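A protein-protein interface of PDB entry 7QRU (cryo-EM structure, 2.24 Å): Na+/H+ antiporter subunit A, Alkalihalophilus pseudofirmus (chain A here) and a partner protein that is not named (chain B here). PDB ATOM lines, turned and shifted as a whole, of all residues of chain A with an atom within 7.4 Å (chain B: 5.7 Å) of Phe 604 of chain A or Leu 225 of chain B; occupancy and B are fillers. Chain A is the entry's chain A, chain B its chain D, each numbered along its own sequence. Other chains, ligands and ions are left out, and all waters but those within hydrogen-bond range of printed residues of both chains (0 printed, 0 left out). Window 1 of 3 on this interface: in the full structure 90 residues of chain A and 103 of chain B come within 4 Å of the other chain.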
ATOM      1  N   TYR A 597     -17.178  -0.929  11.719  1.00  0.00           N
ATOM      2  CA  TYR A 597     -16.108   0.009  11.454  1.00  0.00           C
ATOM      3  C   TYR A 597     -15.670   0.754  12.700  1.00  0.00           C
ATOM      4  O   TYR A 597     -14.443   0.850  12.946  1.00  0.00           O
ATOM      5  CB  TYR A 597     -16.473   0.980  10.362  1.00  0.00           C
ATOM      6  CG  TYR A 597     -16.974   0.294   9.132  1.00  0.00           C
ATOM      7  CD1 TYR A 597     -16.445  -0.944   8.739  1.00  0.00           C
ATOM      8  CD2 TYR A 597     -17.835   0.969   8.278  1.00  0.00           C
ATOM      9  CE1 TYR A 597     -16.874  -1.557   7.578  1.00  0.00           C
ATOM     10  CE2 TYR A 597     -18.301   0.328   7.156  1.00  0.00           C
ATOM     11  CZ  TYR A 597     -17.804  -0.929   6.789  1.00  0.00           C
ATOM     12  OH  TYR A 597     -18.239  -1.543   5.647  1.00  0.00           O
ATOM     13  N   PHE A 598     -16.612   1.242  13.537  1.00  0.00           N
ATOM     14  CA  PHE A 598     -16.127   1.942  14.725  1.00  0.00           C
ATOM     15  C   PHE A 598     -15.452   0.991  15.699  1.00  0.00           C
ATOM     16  O   PHE A 598     -14.462   1.371  16.283  1.00  0.00           O
ATOM     17  CB  PHE A 598     -17.224   2.637  15.499  1.00  0.00           C
ATOM     18  CG  PHE A 598     -17.690   3.907  14.877  1.00  0.00           C
ATOM     19  CD1 PHE A 598     -16.785   4.910  14.588  1.00  0.00           C
ATOM     20  CD2 PHE A 598     -19.040   4.085  14.661  1.00  0.00           C
ATOM     21  CE1 PHE A 598     -17.262   6.101  14.076  1.00  0.00           C
ATOM     22  CE2 PHE A 598     -19.522   5.297  14.209  1.00  0.00           C
ATOM     23  CZ  PHE A 598     -18.619   6.283  13.892  1.00  0.00           C
ATOM     24  N   ALA A 599     -15.941  -0.256  15.811  1.00  0.00           N
ATOM     25  CA  ALA A 599     -15.309  -1.209  16.715  1.00  0.00           C
ATOM     26  C   ALA A 599     -13.906  -1.618  16.269  1.00  0.00           C
ATOM     27  O   ALA A 599     -13.034  -1.818  17.107  1.00  0.00           O
ATOM     28  CB  ALA A 599     -16.149  -2.418  16.784  1.00  0.00           C
ATOM     29  N   TYR A 600     -13.660  -1.778  14.951  1.00  0.00           N
ATOM     30  CA  TYR A 600     -12.288  -2.009  14.501  1.00  0.00           C
ATOM     31  C   TYR A 600     -11.367  -0.828  14.804  1.00  0.00           C
ATOM     32  O   TYR A 600     -10.300  -0.957  15.377  1.00  0.00           O
ATOM     33  CB  TYR A 600     -12.188  -2.193  13.008  1.00  0.00           C
ATOM     34  CG  TYR A 600     -12.912  -3.369  12.456  1.00  0.00           C
ATOM     35  CD1 TYR A 600     -13.165  -4.488  13.213  1.00  0.00           C
ATOM     36  CD2 TYR A 600     -13.394  -3.327  11.161  1.00  0.00           C
ATOM     37  CE1 TYR A 600     -13.868  -5.561  12.693  1.00  0.00           C
ATOM     38  CE2 TYR A 600     -14.079  -4.401  10.616  1.00  0.00           C
ATOM     39  CZ  TYR A 600     -14.309  -5.528  11.385  1.00  0.00           C
ATOM     40  OH  TYR A 600     -14.987  -6.571  10.830  1.00  0.00           O
ATOM     41  N   MET A 601     -11.806   0.359  14.441  1.00  0.00           N
ATOM     42  CA  MET A 601     -10.980   1.501  14.717  1.00  0.00           C
ATOM     43  C   MET A 601     -10.724   1.719  16.201  1.00  0.00           C
ATOM     44  O   MET A 601      -9.600   1.921  16.594  1.00  0.00           O
ATOM     45  CB  MET A 601     -11.674   2.714  14.131  1.00  0.00           C
ATOM     46  CG  MET A 601     -11.612   2.559  12.653  1.00  0.00           C
ATOM     47  SD  MET A 601     -12.243   4.013  11.683  1.00  0.00           S
ATOM     48  CE  MET A 601     -13.667   4.421  12.649  1.00  0.00           C
ATOM     49  N   THR A 602     -11.733   1.689  17.049  1.00  0.00           N
ATOM     50  CA  THR A 602     -11.534   1.909  18.477  1.00  0.00           C
ATOM     51  C   THR A 602     -10.755   0.768  19.076  1.00  0.00           C
ATOM     52  O   THR A 602      -9.906   1.025  19.931  1.00  0.00           O
ATOM     53  CB  THR A 602     -12.868   2.101  19.198  1.00  0.00           C
ATOM     54  OG1 THR A 602     -13.809   1.115  18.796  1.00  0.00           O
ATOM     55  CG2 THR A 602     -13.504   3.399  18.802  1.00  0.00           C
ATOM     56  N   THR A 603     -10.955  -0.456  18.602  1.00  0.00           N
ATOM     57  CA  THR A 603     -10.151  -1.532  19.184  1.00  0.00           C
ATOM     58  C   THR A 603      -8.659  -1.357  18.881  1.00  0.00           C
ATOM     59  O   THR A 603      -7.795  -1.368  19.769  1.00  0.00           O
ATOM     60  CB  THR A 603     -10.659  -2.878  18.699  1.00  0.00           C
ATOM     61  OG1 THR A 603     -12.021  -3.034  19.137  1.00  0.00           O
ATOM     62  CG2 THR A 603      -9.778  -3.969  19.205  1.00  0.00           C
ATOM     63  N   PHE A 604      -8.385  -0.963  17.657  1.00  0.00           N
ATOM     64  CA  PHE A 604      -7.040  -0.664  17.283  1.00  0.00           C
ATOM     65  C   PHE A 604      -6.475   0.486  18.113  1.00  0.00           C
ATOM     66  O   PHE A 604      -5.439   0.303  18.694  1.00  0.00           O
ATOM     67  CB  PHE A 604      -6.995  -0.431  15.793  1.00  0.00           C
ATOM     68  CG  PHE A 604      -5.668   0.081  15.333  1.00  0.00           C
ATOM     69  CD1 PHE A 604      -4.626  -0.807  15.089  1.00  0.00           C
ATOM     70  CD2 PHE A 604      -5.497   1.442  15.081  1.00  0.00           C
ATOM     71  CE1 PHE A 604      -3.418  -0.309  14.612  1.00  0.00           C
ATOM     72  CE2 PHE A 604      -4.274   1.929  14.625  1.00  0.00           C
ATOM     73  CZ  PHE A 604      -3.245   1.054  14.383  1.00  0.00           C
ATOM     74  N   MET A 605      -7.184   1.595  18.253  1.00  0.00           N
ATOM     75  CA  MET A 605      -6.745   2.651  19.146  1.00  0.00           C
ATOM     76  C   MET A 605      -6.464   2.210  20.588  1.00  0.00           C
ATOM     77  O   MET A 605      -5.492   2.647  21.188  1.00  0.00           O
ATOM     78  CB  MET A 605      -7.837   3.699  19.252  1.00  0.00           C
ATOM     79  CG  MET A 605      -7.859   4.648  18.093  1.00  0.00           C
ATOM     80  SD  MET A 605      -9.461   5.517  18.030  1.00  0.00           S
ATOM     81  CE  MET A 605      -9.362   6.235  19.673  1.00  0.00           C
ATOM     82  N   ILE A 606      -7.279   1.357  21.184  1.00  0.00           N
ATOM     83  CA  ILE A 606      -7.069   0.939  22.560  1.00  0.00           C
ATOM     84  C   ILE A 606      -5.800   0.148  22.686  1.00  0.00           C
ATOM     85  O   ILE A 606      -4.979   0.518  23.550  1.00  0.00           O
ATOM     86  CB  ILE A 606      -8.237   0.099  23.068  1.00  0.00           C
ATOM     87  CG1 ILE A 606      -9.511   0.924  23.222  1.00  0.00           C
ATOM     88  CG2 ILE A 606      -7.950  -0.513  24.381  1.00  0.00           C
ATOM     89  CD1 ILE A 606     -10.641   0.018  23.366  1.00  0.00           C
ATOM     90  N   LEU A 607      -5.592  -0.787  21.766  1.00  0.00           N
ATOM     91  CA  LEU A 607      -4.416  -1.637  21.802  1.00  0.00           C
ATOM     92  C   LEU A 607      -3.133  -0.845  21.552  1.00  0.00           C
ATOM     93  O   LEU A 607      -2.145  -1.052  22.237  1.00  0.00           O
ATOM     94  CB  LEU A 607      -4.557  -2.722  20.736  1.00  0.00           C
ATOM     95  CG  LEU A 607      -5.688  -3.726  20.957  1.00  0.00           C
ATOM     96  CD1 LEU A 607      -5.742  -4.683  19.809  1.00  0.00           C
ATOM     97  CD2 LEU A 607      -5.555  -4.440  22.282  1.00  0.00           C
ATOM     98  N   LEU A 608      -3.155   0.106  20.641  1.00  0.00           N
ATOM     99  CA  LEU A 608      -1.961   0.859  20.355  1.00  0.00           C
ATOM    100  C   LEU A 608      -1.695   1.940  21.402  1.00  0.00           C
ATOM    101  O   LEU A 608      -0.580   2.018  21.925  1.00  0.00           O
ATOM    102  CB  LEU A 608      -2.170   1.424  18.960  1.00  0.00           C
ATOM    103  CG  LEU A 608      -0.968   2.190  18.411  1.00  0.00           C
ATOM    104  CD1 LEU A 608       0.284   1.347  18.464  1.00  0.00           C
ATOM    105  CD2 LEU A 608      -1.266   2.639  17.003  1.00  0.00           C
ATOM    106  N   LEU A 609      -2.711   2.690  21.828  1.00  0.00           N
ATOM    107  CA  LEU A 609      -2.436   3.679  22.879  1.00  0.00           C
ATOM    108  C   LEU A 609      -2.134   2.989  24.177  1.00  0.00           C
ATOM    109  O   LEU A 609      -1.277   3.459  24.952  1.00  0.00           O
ATOM    110  CB  LEU A 609      -3.602   4.644  23.065  1.00  0.00           C
ATOM    111  CG  LEU A 609      -3.903   5.519  21.838  1.00  0.00           C
ATOM    112  CD1 LEU A 609      -5.181   6.241  22.058  1.00  0.00           C
ATOM    113  CD2 LEU A 609      -2.827   6.531  21.614  1.00  0.00           C
ATOM    114  N   GLY A 610      -2.861   1.892  24.421  1.00  0.00           N
ATOM    115  CA  GLY A 610      -2.599   1.089  25.574  1.00  0.00           C
ATOM    116  C   GLY A 610      -1.175   0.568  25.603  1.00  0.00           C
ATOM    117  O   GLY A 610      -0.511   0.669  26.626  1.00  0.00           O
ATOM    118  N   LEU B 213      -0.772  10.209  14.948  1.00  0.00           N
ATOM    119  CA  LEU B 213      -0.660   9.266  13.872  1.00  0.00           C
ATOM    120  C   LEU B 213      -2.020   8.672  13.511  1.00  0.00           C
ATOM    121  O   LEU B 213      -2.340   8.611  12.346  1.00  0.00           O
ATOM    122  CB  LEU B 213       0.299   8.164  14.235  1.00  0.00           C
ATOM    123  CG  LEU B 213       0.289   7.066  13.188  1.00  0.00           C
ATOM    124  CD1 LEU B 213       0.639   7.670  11.821  1.00  0.00           C
ATOM    125  CD2 LEU B 213       1.329   6.052  13.598  1.00  0.00           C
ATOM    126  N   VAL B 214      -2.811   8.267  14.485  1.00  0.00           N
ATOM    127  CA  VAL B 214      -4.072   7.678  14.179  1.00  0.00           C
ATOM    128  C   VAL B 214      -4.996   8.700  13.512  1.00  0.00           C
ATOM    129  O   VAL B 214      -5.876   8.343  12.776  1.00  0.00           O
ATOM    130  CB  VAL B 214      -4.713   7.195  15.516  1.00  0.00           C
ATOM    131  CG1 VAL B 214      -6.161   6.800  15.350  1.00  0.00           C
ATOM    132  CG2 VAL B 214      -3.946   6.078  16.133  1.00  0.00           C
ATOM    133  N   ALA B 217      -3.845   9.171  10.089  1.00  0.00           N
ATOM    134  CA  ALA B 217      -3.967   7.897   9.405  1.00  0.00           C
ATOM    135  C   ALA B 217      -5.402   7.639   9.035  1.00  0.00           C
ATOM    136  O   ALA B 217      -5.612   7.056   7.976  1.00  0.00           O
ATOM    137  CB  ALA B 217      -3.463   6.788  10.235  1.00  0.00           C
ATOM    138  N   MET B 218      -6.382   8.106   9.822  1.00  0.00           N
ATOM    139  CA  MET B 218      -7.787   7.934   9.443  1.00  0.00           C
ATOM    140  C   MET B 218      -8.111   8.823   8.250  1.00  0.00           C
ATOM    141  O   MET B 218      -8.766   8.361   7.327  1.00  0.00           O
ATOM    142  CB  MET B 218      -8.781   8.278  10.557  1.00  0.00           C
ATOM    143  CG  MET B 218      -8.723   7.330  11.730  1.00  0.00           C
ATOM    144  SD  MET B 218      -9.924   7.769  13.072  1.00  0.00           S
ATOM    145  CE  MET B 218     -11.458   7.403  12.229  1.00  0.00           C
ATOM    146  N   LYS B 219      -7.672  10.079   8.252  1.00  0.00           N
ATOM    147  CA  LYS B 219      -7.864  10.999   7.123  1.00  0.00           C
ATOM    148  C   LYS B 219      -7.040  10.586   5.889  1.00  0.00           C
ATOM    149  O   LYS B 219      -7.502  10.729   4.759  1.00  0.00           O
ATOM    150  CB  LYS B 219      -7.550  12.419   7.602  1.00  0.00           C
ATOM    151  CG  LYS B 219      -8.461  12.872   8.743  1.00  0.00           C
ATOM    152  CD  LYS B 219      -8.062  14.210   9.349  1.00  0.00           C
ATOM    153  CE  LYS B 219      -8.845  14.690  10.566  1.00  0.00           C
ATOM    154  NZ  LYS B 219     -10.308  14.470  10.559  1.00  0.00           N
ATOM    155  N   GLY B 221      -6.183   7.276   5.072  1.00  0.00           N
ATOM    156  CA  GLY B 221      -6.670   6.020   4.544  1.00  0.00           C
ATOM    157  C   GLY B 221      -5.704   4.858   4.842  1.00  0.00           C
ATOM    158  O   GLY B 221      -5.704   3.912   4.088  1.00  0.00           O
ATOM    159  N   LEU B 222      -4.906   4.924   5.890  1.00  0.00           N
ATOM    160  CA  LEU B 222      -4.090   3.800   6.291  1.00  0.00           C
ATOM    161  C   LEU B 222      -4.897   2.717   6.966  1.00  0.00           C
ATOM    162  O   LEU B 222      -5.976   2.950   7.443  1.00  0.00           O
ATOM    163  CB  LEU B 222      -3.001   4.232   7.256  1.00  0.00           C
ATOM    164  CG  LEU B 222      -2.145   5.335   6.665  1.00  0.00           C
ATOM    165  CD1 LEU B 222      -0.900   5.505   7.484  1.00  0.00           C
ATOM    166  CD2 LEU B 222      -1.814   5.048   5.198  1.00  0.00           C
ATOM    167  N   PHE B 223      -4.412   1.488   6.889  1.00  0.00           N
ATOM    168  CA  PHE B 223      -5.020   0.367   7.592  1.00  0.00           C
ATOM    169  C   PHE B 223      -4.692   0.495   9.070  1.00  0.00           C
ATOM    170  O   PHE B 223      -3.616   0.956   9.339  1.00  0.00           O
ATOM    171  CB  PHE B 223      -4.414  -0.933   7.093  1.00  0.00           C
ATOM    172  CG  PHE B 223      -4.824  -2.183   7.785  1.00  0.00           C
ATOM    173  CD1 PHE B 223      -4.179  -2.580   8.951  1.00  0.00           C
ATOM    174  CD2 PHE B 223      -5.890  -2.922   7.287  1.00  0.00           C
ATOM    175  CE1 PHE B 223      -4.596  -3.728   9.606  1.00  0.00           C
ATOM    176  CE2 PHE B 223      -6.236  -4.118   7.893  1.00  0.00           C
ATOM    177  CZ  PHE B 223      -5.579  -4.518   9.050  1.00  0.00           C
ATOM    178  N   PRO B 224      -5.565   0.103  10.024  1.00  0.00           N
ATOM    179  CA  PRO B 224      -6.952  -0.341   9.715  1.00  0.00           C
ATOM    180  C   PRO B 224      -8.011   0.727   9.949  1.00  0.00           C
ATOM    181  O   PRO B 224      -8.880   0.626  10.803  1.00  0.00           O
ATOM    182  CB  PRO B 224      -7.107  -1.435  10.778  1.00  0.00           C
ATOM    183  CG  PRO B 224      -6.454  -0.834  11.959  1.00  0.00           C
ATOM    184  CD  PRO B 224      -5.181  -0.175  11.423  1.00  0.00           C
ATOM    185  N   LEU B 225      -7.832   1.851   9.300  1.00  0.00           N
ATOM    186  CA  LEU B 225      -8.618   3.018   9.602  1.00  0.00           C
ATOM    187  C   LEU B 225      -9.208   3.598   8.335  1.00  0.00           C
ATOM    188  O   LEU B 225      -9.442   4.816   8.310  1.00  0.00           O
ATOM    189  CB  LEU B 225      -7.647   4.018  10.248  1.00  0.00           C
ATOM    190  CG  LEU B 225      -7.141   3.573  11.599  1.00  0.00           C
ATOM    191  CD1 LEU B 225      -5.973   4.438  12.032  1.00  0.00           C
ATOM    192  CD2 LEU B 225      -8.321   3.617  12.542  1.00  0.00           C
ATOM    193  N   TYR B 226      -9.477   2.771   7.328  1.00  0.00           N
ATOM    194  CA  TYR B 226      -9.885   3.289   6.034  1.00  0.00           C
ATOM    195  C   TYR B 226     -11.342   2.991   5.681  1.00  0.00           C
ATOM    196  O   TYR B 226     -11.683   3.145   4.543  1.00  0.00           O
ATOM    197  CB  TYR B 226      -8.967   2.765   4.930  1.00  0.00           C
ATOM    198  CG  TYR B 226      -8.721   1.301   4.899  1.00  0.00           C
ATOM    199  CD1 TYR B 226      -9.744   0.413   4.656  1.00  0.00           C
ATOM    200  CD2 TYR B 226      -7.437   0.797   4.987  1.00  0.00           C
ATOM    201  CE1 TYR B 226      -9.544  -0.951   4.678  1.00  0.00           C
ATOM    202  CE2 TYR B 226      -7.195  -0.580   4.932  1.00  0.00           C
ATOM    203  CZ  TYR B 226      -8.255  -1.450   4.768  1.00  0.00           C
ATOM    204  OH  TYR B 226      -8.125  -2.804   4.677  1.00  0.00           O
ATOM    205  N   PHE B 227     -12.123   2.352   6.528  1.00  0.00           N
ATOM    206  CA  PHE B 227     -13.389   1.746   6.106  1.00  0.00           C
ATOM    207  C   PHE B 227     -14.331   2.785   5.467  1.00  0.00           C
ATOM    208  O   PHE B 227     -15.135   2.489   4.620  1.00  0.00           O
ATOM    209  CB  PHE B 227     -14.072   1.180   7.351  1.00  0.00           C
ATOM    210  CG  PHE B 227     -13.168   0.233   8.047  1.00  0.00           C
ATOM    211  CD1 PHE B 227     -12.843  -0.947   7.424  1.00  0.00           C
ATOM    212  CD2 PHE B 227     -12.583   0.562   9.273  1.00  0.00           C
ATOM    213  CE1 PHE B 227     -11.935  -1.821   7.992  1.00  0.00           C
ATOM    214  CE2 PHE B 227     -11.712  -0.325   9.864  1.00  0.00           C
ATOM    215  CZ  PHE B 227     -11.385  -1.512   9.214  1.00  0.00           C
ATOM    216  N   TRP B 228     -14.181   4.025   5.863  1.00  0.00           N
ATOM    217  CA  TRP B 228     -14.923   5.100   5.275  1.00  0.00           C
ATOM    218  C   TRP B 228     -14.715   5.273   3.775  1.00  0.00           C
ATOM    219  O   TRP B 228     -15.593   5.878   3.196  1.00  0.00           O
ATOM    220  CB  TRP B 228     -14.548   6.410   5.954  1.00  0.00           C
ATOM    221  CG  TRP B 228     -13.135   6.795   5.942  1.00  0.00           C
ATOM    222  CD1 TRP B 228     -12.166   6.437   6.823  1.00  0.00           C
ATOM    223  CD2 TRP B 228     -12.521   7.621   4.946  1.00  0.00           C
ATOM    224  NE1 TRP B 228     -10.983   7.034   6.477  1.00  0.00           N
ATOM    225  CE2 TRP B 228     -11.161   7.772   5.328  1.00  0.00           C
ATOM    226  CE3 TRP B 228     -12.956   8.155   3.731  1.00  0.00           C
ATOM    227  CZ2 TRP B 228     -10.238   8.463   4.533  1.00  0.00           C
ATOM    228  CZ3 TRP B 228     -12.059   8.865   2.941  1.00  0.00           C
ATOM    229  CH2 TRP B 228     -10.712   9.043   3.367  1.00  0.00           C
ATOM    230  N   LEU B 274       6.476   1.924  13.741  1.00  0.00           N
ATOM    231  CA  LEU B 274       5.045   1.776  13.673  1.00  0.00           C
ATOM    232  C   LEU B 274       4.530   2.241  12.326  1.00  0.00           C
ATOM    233  O   LEU B 274       3.779   1.529  11.698  1.00  0.00           O
ATOM    234  CB  LEU B 274       4.499   2.566  14.849  1.00  0.00           C
ATOM    235  CG  LEU B 274       3.014   2.812  14.873  1.00  0.00           C
ATOM    236  CD1 LEU B 274       2.282   1.500  14.900  1.00  0.00           C
ATOM    237  CD2 LEU B 274       2.747   3.585  16.121  1.00  0.00           C
ATOM    238  N   LEU B 278       2.295   0.003   9.461  1.00  0.00           N
ATOM    239  CA  LEU B 278       0.988   0.329   8.921  1.00  0.00           C
ATOM    240  C   LEU B 278       1.136   0.516   7.413  1.00  0.00           C
ATOM    241  O   LEU B 278       0.237   0.134   6.731  1.00  0.00           O
ATOM    242  CB  LEU B 278       0.416   1.608   9.570  1.00  0.00           C
ATOM    243  CG  LEU B 278       0.272   1.505  11.086  1.00  0.00           C
ATOM    244  CD1 LEU B 278      -0.145   2.829  11.615  1.00  0.00           C
ATOM    245  CD2 LEU B 278      -0.723   0.403  11.441  1.00  0.00           C
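NE1 of Trp 228 of chain B sits at hydrogen-bond distance from O of Leu 225 of chain B (3.3 Å). The backbone carbonyl oxygen (O) of Met 218 of chain B is in hydrogen-bond range of the indole nitrogen (NE1) of Trp 228 of chain B, 2.7 Å away.
Phe 227 of chain B touches Tyr 597 of chain A (CB to CD1, 3.5 Å). Tyr 600 of chain A touches Phe 227 of chain B. Met 601 of chain A touches Met 218 of chain B. Met 601 of chain A touches Pro 224 of chain B. Met 601 of chain A touches Leu 225 of chain B (CG to CD2, 3.5 Å). Pro 224 of chain B touches Phe 604 of chain A. Leu 225 of chain B touches Phe 604 of chain A. CD2 of Leu 278 of chain B touches CZ of Phe 604 of chain A, at 3.9 Å. Met 605 of chain A touches Val 214 of chain B.
Printed residues of chain B within 4 Å of Tyr 597 of chain A: Phe 227. Of the printed residues of chain B, Tyr 600 of chain A touches Phe 227. Of the printed residues of chain B, Phe 604 of chain A touches Pro 224 (3.6 Å), Leu 225 (3.99 Å) and Leu 278 (3.9 Å). Printed residues of chain B within 4 Å of Met 605 of chain A: Val 214 (3.9 Å). Printed residues of chain A within 4 Å of Met 218 of chain B: Met 601 (3.5 Å). Leu 274 of chain B touches none of the printed residues of chain A.
Hydrophobic or aromatic side chains of chain A within 4 Å of the printed part of chain B: Tyr 597, Tyr 600, Met 601, Phe 604 and Met 605. Of the 15 printed residues of chain B, 6 touch a printed residue of chain A. Hydrophobic or aromatic side chains of chain B within 4 Å of the printed part of chain A: Val 214, Met 218, Pro 224, Leu 225, Phe 227 and Leu 278. Among the printed residues, 9 pairs touch across the chains.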
